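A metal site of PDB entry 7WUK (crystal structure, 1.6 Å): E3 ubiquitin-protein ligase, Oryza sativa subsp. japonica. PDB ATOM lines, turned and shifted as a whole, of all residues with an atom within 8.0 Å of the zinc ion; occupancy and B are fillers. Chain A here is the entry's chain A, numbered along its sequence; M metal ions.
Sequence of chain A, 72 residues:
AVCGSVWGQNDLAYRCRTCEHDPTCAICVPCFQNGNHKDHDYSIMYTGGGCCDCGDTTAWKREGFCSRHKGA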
ATOM      1  N   ARG A  15      19.041   5.543   1.221  1.00  0.00           N
ATOM      2  CA  ARG A  15      18.816   4.139   1.513  1.00  0.00           C
ATOM      3  C   ARG A  15      19.097   3.938   2.999  1.00  0.00           C
ATOM      4  O   ARG A  15      19.960   4.622   3.541  1.00  0.00           O
ATOM      5  CB  ARG A  15      19.704   3.282   0.605  1.00  0.00           C
ATOM      6  CG  ARG A  15      19.237   3.423  -0.838  1.00  0.00           C
ATOM      7  CD  ARG A  15      19.591   2.283  -1.668  1.00  0.00           C
ATOM      8  NE  ARG A  15      19.536   2.509  -3.084  1.00  0.00           N
ATOM      9  CZ  ARG A  15      18.465   2.430  -3.855  1.00  0.00           C
ATOM     10  NH1 ARG A  15      17.251   2.248  -3.362  1.00  0.00           N
ATOM     11  NH2 ARG A  15      18.612   2.494  -5.164  1.00  0.00           N
ATOM     12  N   CYS A  16      18.385   3.023   3.592  1.00  0.00           N
ATOM     13  CA  CYS A  16      18.680   2.627   4.988  1.00  0.00           C
ATOM     14  C   CYS A  16      18.553   1.131   5.054  1.00  0.00           C
ATOM     15  O   CYS A  16      17.434   0.619   5.010  1.00  0.00           O
ATOM     16  CB  CYS A  16      17.836   3.338   6.039  1.00  0.00           C
ATOM     17  SG  CYS A  16      18.425   2.869   7.686  1.00  0.00           S
ATOM     18  N   ARG A  17      19.699   0.512   5.078  1.00  0.00           N
ATOM     19  CA  ARG A  17      19.680  -0.935   5.172  1.00  0.00           C
ATOM     20  C   ARG A  17      18.975  -1.581   6.470  1.00  0.00           C
ATOM     21  O   ARG A  17      18.443  -2.740   6.596  1.00  0.00           O
ATOM     22  CB  ARG A  17      21.061  -1.537   4.952  1.00  0.00           C
ATOM     23  CG  ARG A  17      21.753  -1.048   3.718  1.00  0.00           C
ATOM     24  CD  ARG A  17      20.971  -1.201   2.470  1.00  0.00           C
ATOM     25  NE  ARG A  17      21.677  -0.586   1.351  1.00  0.00           N
ATOM     26  CZ  ARG A  17      21.162  -0.433   0.144  1.00  0.00           C
ATOM     27  NH1 ARG A  17      19.918  -0.830  -0.100  1.00  0.00           N
ATOM     28  NH2 ARG A  17      21.921   0.090  -0.809  1.00  0.00           N
ATOM     29  N   THR A  18      19.041  -0.749   7.535  1.00  0.00           N
ATOM     30  CA  THR A  18      18.375  -1.080   8.798  1.00  0.00           C
ATOM     31  C   THR A  18      16.833  -1.136   8.650  1.00  0.00           C
ATOM     32  O   THR A  18      16.201  -2.038   9.221  1.00  0.00           O
ATOM     33  CB  THR A  18      18.806  -0.094   9.893  1.00  0.00           C
ATOM     34  OG1 THR A  18      20.249  -0.075   9.941  1.00  0.00           O
ATOM     35  CG2 THR A  18      18.250  -0.465  11.230  1.00  0.00           C
ATOM     36  N   CYS A  19      16.274  -0.169   7.901  1.00  0.00           N
ATOM     37  CA  CYS A  19      14.803   0.068   7.777  1.00  0.00           C
ATOM     38  C   CYS A  19      14.185  -0.618   6.556  1.00  0.00           C
ATOM     39  O   CYS A  19      12.972  -0.829   6.573  1.00  0.00           O
ATOM     40  CB  CYS A  19      14.526   1.558   7.724  1.00  0.00           C
ATOM     41  SG  CYS A  19      14.849   2.414   9.314  1.00  0.00           S
ATOM     42  N   GLU A  20      14.950  -0.927   5.522  1.00  0.00           N
ATOM     43  CA  GLU A  20      14.362  -1.308   4.226  1.00  0.00           C
ATOM     44  C   GLU A  20      13.804  -2.715   4.326  1.00  0.00           C
ATOM     45  O   GLU A  20      14.360  -3.509   5.119  1.00  0.00           O
ATOM     46  CB  GLU A  20      15.401  -1.256   3.124  1.00  0.00           C
ATOM     47  CG  GLU A  20      16.428  -2.396   3.192  1.00  0.00           C
ATOM     48  CD  GLU A  20      17.615  -2.354   2.215  1.00  0.00           C
ATOM     49  OE1 GLU A  20      17.955  -1.233   1.801  1.00  0.00           O
ATOM     50  OE2 GLU A  20      18.251  -3.399   1.955  1.00  0.00           O
ATOM     51  N   ILE A  27      13.994   6.495   0.809  1.00  0.00           N
ATOM     52  CA  ILE A  27      13.148   7.602   1.326  1.00  0.00           C
ATOM     53  C   ILE A  27      13.767   8.932   0.940  1.00  0.00           C
ATOM     54  O   ILE A  27      14.980   9.028   0.767  1.00  0.00           O
ATOM     55  CB  ILE A  27      12.846   7.543   2.826  1.00  0.00           C
ATOM     56  CG1 ILE A  27      14.089   7.656   3.709  1.00  0.00           C
ATOM     57  CG2 ILE A  27      12.047   6.278   3.144  1.00  0.00           C
ATOM     58  CD1 ILE A  27      13.746   7.795   5.171  1.00  0.00           C
ATOM     59  N   PHE A  32      14.016  11.314   5.664  1.00  0.00           N
ATOM     60  CA  PHE A  32      15.206  10.869   6.423  1.00  0.00           C
ATOM     61  C   PHE A  32      15.466  11.835   7.577  1.00  0.00           C
ATOM     62  O   PHE A  32      15.665  11.367   8.736  1.00  0.00           O
ATOM     63  CB  PHE A  32      16.434  10.729   5.523  1.00  0.00           C
ATOM     64  CG  PHE A  32      17.590  10.215   6.330  1.00  0.00           C
ATOM     65  CD1 PHE A  32      17.742   8.848   6.549  1.00  0.00           C
ATOM     66  CD2 PHE A  32      18.474  11.094   6.904  1.00  0.00           C
ATOM     67  CE1 PHE A  32      18.765   8.392   7.368  1.00  0.00           C
ATOM     68  CE2 PHE A  32      19.539  10.635   7.678  1.00  0.00           C
ATOM     69  CZ  PHE A  32      19.653   9.289   7.910  1.00  0.00           C
ATOM     70  N   GLY A  35      13.180  11.625  10.617  1.00  0.00           N
ATOM     71  CA  GLY A  35      13.111  10.319  11.286  1.00  0.00           C
ATOM     72  C   GLY A  35      14.355  10.031  12.100  1.00  0.00           C
ATOM     73  O   GLY A  35      15.272  10.877  12.204  1.00  0.00           O
ATOM     74  N   ASN A  36      14.344   8.845  12.677  1.00  0.00           N
ATOM     75  CA  ASN A  36      15.345   8.404  13.674  1.00  0.00           C
ATOM     76  C   ASN A  36      16.155   7.251  13.067  1.00  0.00           C
ATOM     77  O   ASN A  36      15.641   6.126  13.037  1.00  0.00           O
ATOM     78  CB  ASN A  36      14.607   8.019  14.935  1.00  0.00           C
ATOM     79  CG  ASN A  36      13.791   9.160  15.492  1.00  0.00           C
ATOM     80  OD1 ASN A  36      14.185  10.324  15.385  1.00  0.00           O
ATOM     81  ND2 ASN A  36      12.623   8.833  16.015  1.00  0.00           N
ATOM     82  N   HIS A  37      17.372   7.538  12.639  1.00  0.00           N
ATOM     83  CA  HIS A  37      18.249   6.498  12.035  1.00  0.00           C
ATOM     84  C   HIS A  37      19.607   6.511  12.695  1.00  0.00           C
ATOM     85  O   HIS A  37      20.584   6.158  12.037  1.00  0.00           O
ATOM     86  CB  HIS A  37      18.298   6.685  10.518  1.00  0.00           C
ATOM     87  CG  HIS A  37      16.951   6.680   9.878  1.00  0.00           C
ATOM     88  ND1 HIS A  37      16.361   5.524   9.412  1.00  0.00           N
ATOM     89  CD2 HIS A  37      16.086   7.686   9.610  1.00  0.00           C
ATOM     90  CE1 HIS A  37      15.172   5.809   8.903  1.00  0.00           C
ATOM     91  NE2 HIS A  37      14.957   7.103   9.054  1.00  0.00           N
ATOM     92  N   LYS A  38      19.691   6.954  13.937  1.00  0.00           N
ATOM     93  CA  LYS A  38      20.972   6.954  14.660  1.00  0.00           C
ATOM     94  C   LYS A  38      21.446   5.483  14.791  1.00  0.00           C
ATOM     95  O   LYS A  38      20.699   4.502  15.194  1.00  0.00           O
ATOM     96  CB  LYS A  38      20.889   7.661  16.009  1.00  0.00           C
ATOM     97  CG  LYS A  38      20.381   9.083  16.024  1.00  0.00           C
ATOM     98  CD  LYS A  38      20.895   9.983  14.964  1.00  0.00           C
ATOM     99  CE  LYS A  38      20.396  11.393  15.167  1.00  0.00           C
ATOM    100  NZ  LYS A  38      20.767  11.890  16.514  1.00  0.00           N
ATOM    101  N   ASP A  39      22.678   5.317  14.417  1.00  0.00           N
ATOM    102  CA  ASP A  39      23.388   4.023  14.340  1.00  0.00           C
ATOM    103  C   ASP A  39      22.762   3.086  13.311  1.00  0.00           C
ATOM    104  O   ASP A  39      23.104   1.908  13.304  1.00  0.00           O
ATOM    105  CB  ASP A  39      23.442   3.318  15.678  1.00  0.00           C
ATOM    106  CG  ASP A  39      24.615   3.747  16.552  1.00  0.00           C
ATOM    107  OD1 ASP A  39      25.743   4.024  16.000  1.00  0.00           O
ATOM    108  OD2 ASP A  39      24.405   3.778  17.795  1.00  0.00           O
ATOM    109  N   HIS A  40      21.931   3.595  12.411  1.00  0.00           N
ATOM    110  CA  HIS A  40      21.470   2.725  11.303  1.00  0.00           C
ATOM    111  C   HIS A  40      22.529   2.689  10.218  1.00  0.00           C
ATOM    112  O   HIS A  40      23.368   3.603  10.115  1.00  0.00           O
ATOM    113  CB  HIS A  40      20.190   3.276  10.718  1.00  0.00           C
ATOM    114  CG  HIS A  40      19.010   3.131  11.589  1.00  0.00           C
ATOM    115  ND1 HIS A  40      17.735   3.111  11.096  1.00  0.00           N
ATOM    116  CD2 HIS A  40      18.909   2.921  12.928  1.00  0.00           C
ATOM    117  CE1 HIS A  40      16.903   2.967  12.090  1.00  0.00           C
ATOM    118  NE2 HIS A  40      17.587   2.756  13.229  1.00  0.00           N
ATOM    119  N   ASP A  41      22.441   1.670   9.344  1.00  0.00           N
ATOM    120  CA  ASP A  41      23.325   1.560   8.173  1.00  0.00           C
ATOM    121  C   ASP A  41      22.673   2.316   7.024  1.00  0.00           C
ATOM    122  O   ASP A  41      22.053   1.716   6.147  1.00  0.00           O
ATOM    123  CB  ASP A  41      23.461   0.104   7.770  1.00  0.00           C
ATOM    124  CG  ASP A  41      24.328  -0.116   6.532  1.00  0.00           C
ATOM    125  OD1 ASP A  41      25.113   0.804   6.174  1.00  0.00           O
ATOM    126  OD2 ASP A  41      24.246  -1.245   5.993  1.00  0.00           O
ATOM    127  N   TYR A  42      22.765   3.624   7.054  1.00  0.00           N
ATOM    128  CA  TYR A  42      22.175   4.445   5.976  1.00  0.00           C
ATOM    129  C   TYR A  42      23.256   5.080   5.104  1.00  0.00           C
ATOM    130  O   TYR A  42      24.412   5.262   5.472  1.00  0.00           O
ATOM    131  CB  TYR A  42      21.283   5.505   6.595  1.00  0.00           C
ATOM    132  CG  TYR A  42      21.991   6.551   7.404  1.00  0.00           C
ATOM    133  CD1 TYR A  42      22.576   7.642   6.795  1.00  0.00           C
ATOM    134  CD2 TYR A  42      22.013   6.474   8.791  1.00  0.00           C
ATOM    135  CE1 TYR A  42      23.228   8.608   7.527  1.00  0.00           C
ATOM    136  CE2 TYR A  42      22.685   7.420   9.539  1.00  0.00           C
ATOM    137  CZ  TYR A  42      23.238   8.527   8.912  1.00  0.00           C
ATOM    138  OH  TYR A  42      23.901   9.455   9.661  1.00  0.00           O
ATOM    139  N   TRP A  60       9.036  -0.484   4.213  1.00  0.00           N
ATOM    140  CA  TRP A  60       9.913   0.217   5.184  1.00  0.00           C
ATOM    141  C   TRP A  60       9.439  -0.109   6.608  1.00  0.00           C
ATOM    142  O   TRP A  60       8.222  -0.048   6.888  1.00  0.00           O
ATOM    143  CB  TRP A  60       9.833   1.726   4.952  1.00  0.00           C
ATOM    144  CG  TRP A  60      10.976   2.555   5.430  1.00  0.00           C
ATOM    145  CD1 TRP A  60      11.010   3.308   6.564  1.00  0.00           C
ATOM    146  CD2 TRP A  60      12.231   2.779   4.752  1.00  0.00           C
ATOM    147  NE1 TRP A  60      12.170   4.025   6.622  1.00  0.00           N
ATOM    148  CE2 TRP A  60      12.952   3.704   5.541  1.00  0.00           C
ATOM    149  CE3 TRP A  60      12.814   2.293   3.586  1.00  0.00           C
ATOM    150  CZ2 TRP A  60      14.203   4.160   5.184  1.00  0.00           C
ATOM    151  CZ3 TRP A  60      14.079   2.722   3.255  1.00  0.00           C
ATOM    152  CH2 TRP A  60      14.763   3.643   4.049  1.00  0.00           C
ATOM    153  N   LYS A  61      10.368  -0.317   7.527  1.00  0.00           N
ATOM    154  CA  LYS A  61      10.000  -0.619   8.943  1.00  0.00           C
ATOM    155  C   LYS A  61       9.329   0.600   9.580  1.00  0.00           C
ATOM    156  O   LYS A  61       9.771   1.719   9.365  1.00  0.00           O
ATOM    157  CB  LYS A  61      11.256  -1.063   9.712  1.00  0.00           C
ATOM    158  CG  LYS A  61      11.753  -2.416   9.244  1.00  0.00           C
ATOM    159  CD  LYS A  61      12.971  -2.948   9.940  1.00  0.00           C
ATOM    160  CE  LYS A  61      13.766  -3.891   9.052  1.00  0.00           C
ATOM    161  NZ  LYS A  61      14.989  -4.371   9.740  1.00  0.00           N
ATOM    162  N   GLU A  63       9.495   1.830  12.520  1.00  0.00           N
ATOM    163  CA  GLU A  63      10.388   2.618  13.408  1.00  0.00           C
ATOM    164  C   GLU A  63      11.225   3.607  12.576  1.00  0.00           C
ATOM    165  O   GLU A  63      11.747   4.581  13.144  1.00  0.00           O
ATOM    166  CB  GLU A  63      11.191   1.634  14.247  1.00  0.00           C
ATOM    167  CG  GLU A  63      10.303   0.959  15.287  1.00  0.00           C
ATOM    168  CD  GLU A  63       9.227   1.815  15.973  1.00  0.00           C
ATOM    169  OE1 GLU A  63       9.572   2.508  16.958  1.00  0.00           O
ATOM    170  OE2 GLU A  63       8.041   1.810  15.521  1.00  0.00           O
ATOM    171  N   GLY A  64      11.259   3.390  11.255  1.00  0.00           N
ATOM    172  CA  GLY A  64      11.986   4.246  10.316  1.00  0.00           C
ATOM    173  C   GLY A  64      11.101   5.274   9.631  1.00  0.00           C
ATOM    174  O   GLY A  64      11.632   5.969   8.801  1.00  0.00           O
ATOM    175  N   PHE A  65       9.825   5.394   9.996  1.00  0.00           N
ATOM    176  CA  PHE A  65       8.940   6.432   9.433  1.00  0.00           C
ATOM    177  C   PHE A  65       9.294   7.778  10.049  1.00  0.00           C
ATOM    178  O   PHE A  65       9.591   7.854  11.309  1.00  0.00           O
ATOM    179  CB  PHE A  65       7.457   6.132   9.700  1.00  0.00           C
ATOM    180  CG  PHE A  65       6.884   4.917   9.030  1.00  0.00           C
ATOM    181  CD1 PHE A  65       7.598   4.180   8.097  1.00  0.00           C
ATOM    182  CD2 PHE A  65       5.607   4.482   9.350  1.00  0.00           C
ATOM    183  CE1 PHE A  65       7.046   3.062   7.497  1.00  0.00           C
ATOM    184  CE2 PHE A  65       5.054   3.373   8.728  1.00  0.00           C
ATOM    185  CZ  PHE A  65       5.772   2.668   7.790  1.00  0.00           C
HETATM  186 ZN    ZN M   1      16.906   3.506   9.241  1.00  0.00          ZN
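SG of Cys 16 sits close to N of Thr 18. N of Lys 61 sits at hydrogen-bond distance from O of Cys 19 (2.8 Å).
Within 4 Å of the zinc ion: Cys 16, Cys 19, His 37 and His 40. Along chain A the residues within 4 Å of the zinc ion span positions 16 to 40.
The zinc ion is bound by ND1 of His 40 (2.1 Å), ND1 of His 37 (2.1 Å), SG of Cys 16 (2.3 Å) and SG of Cys 19 (2.3 Å).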
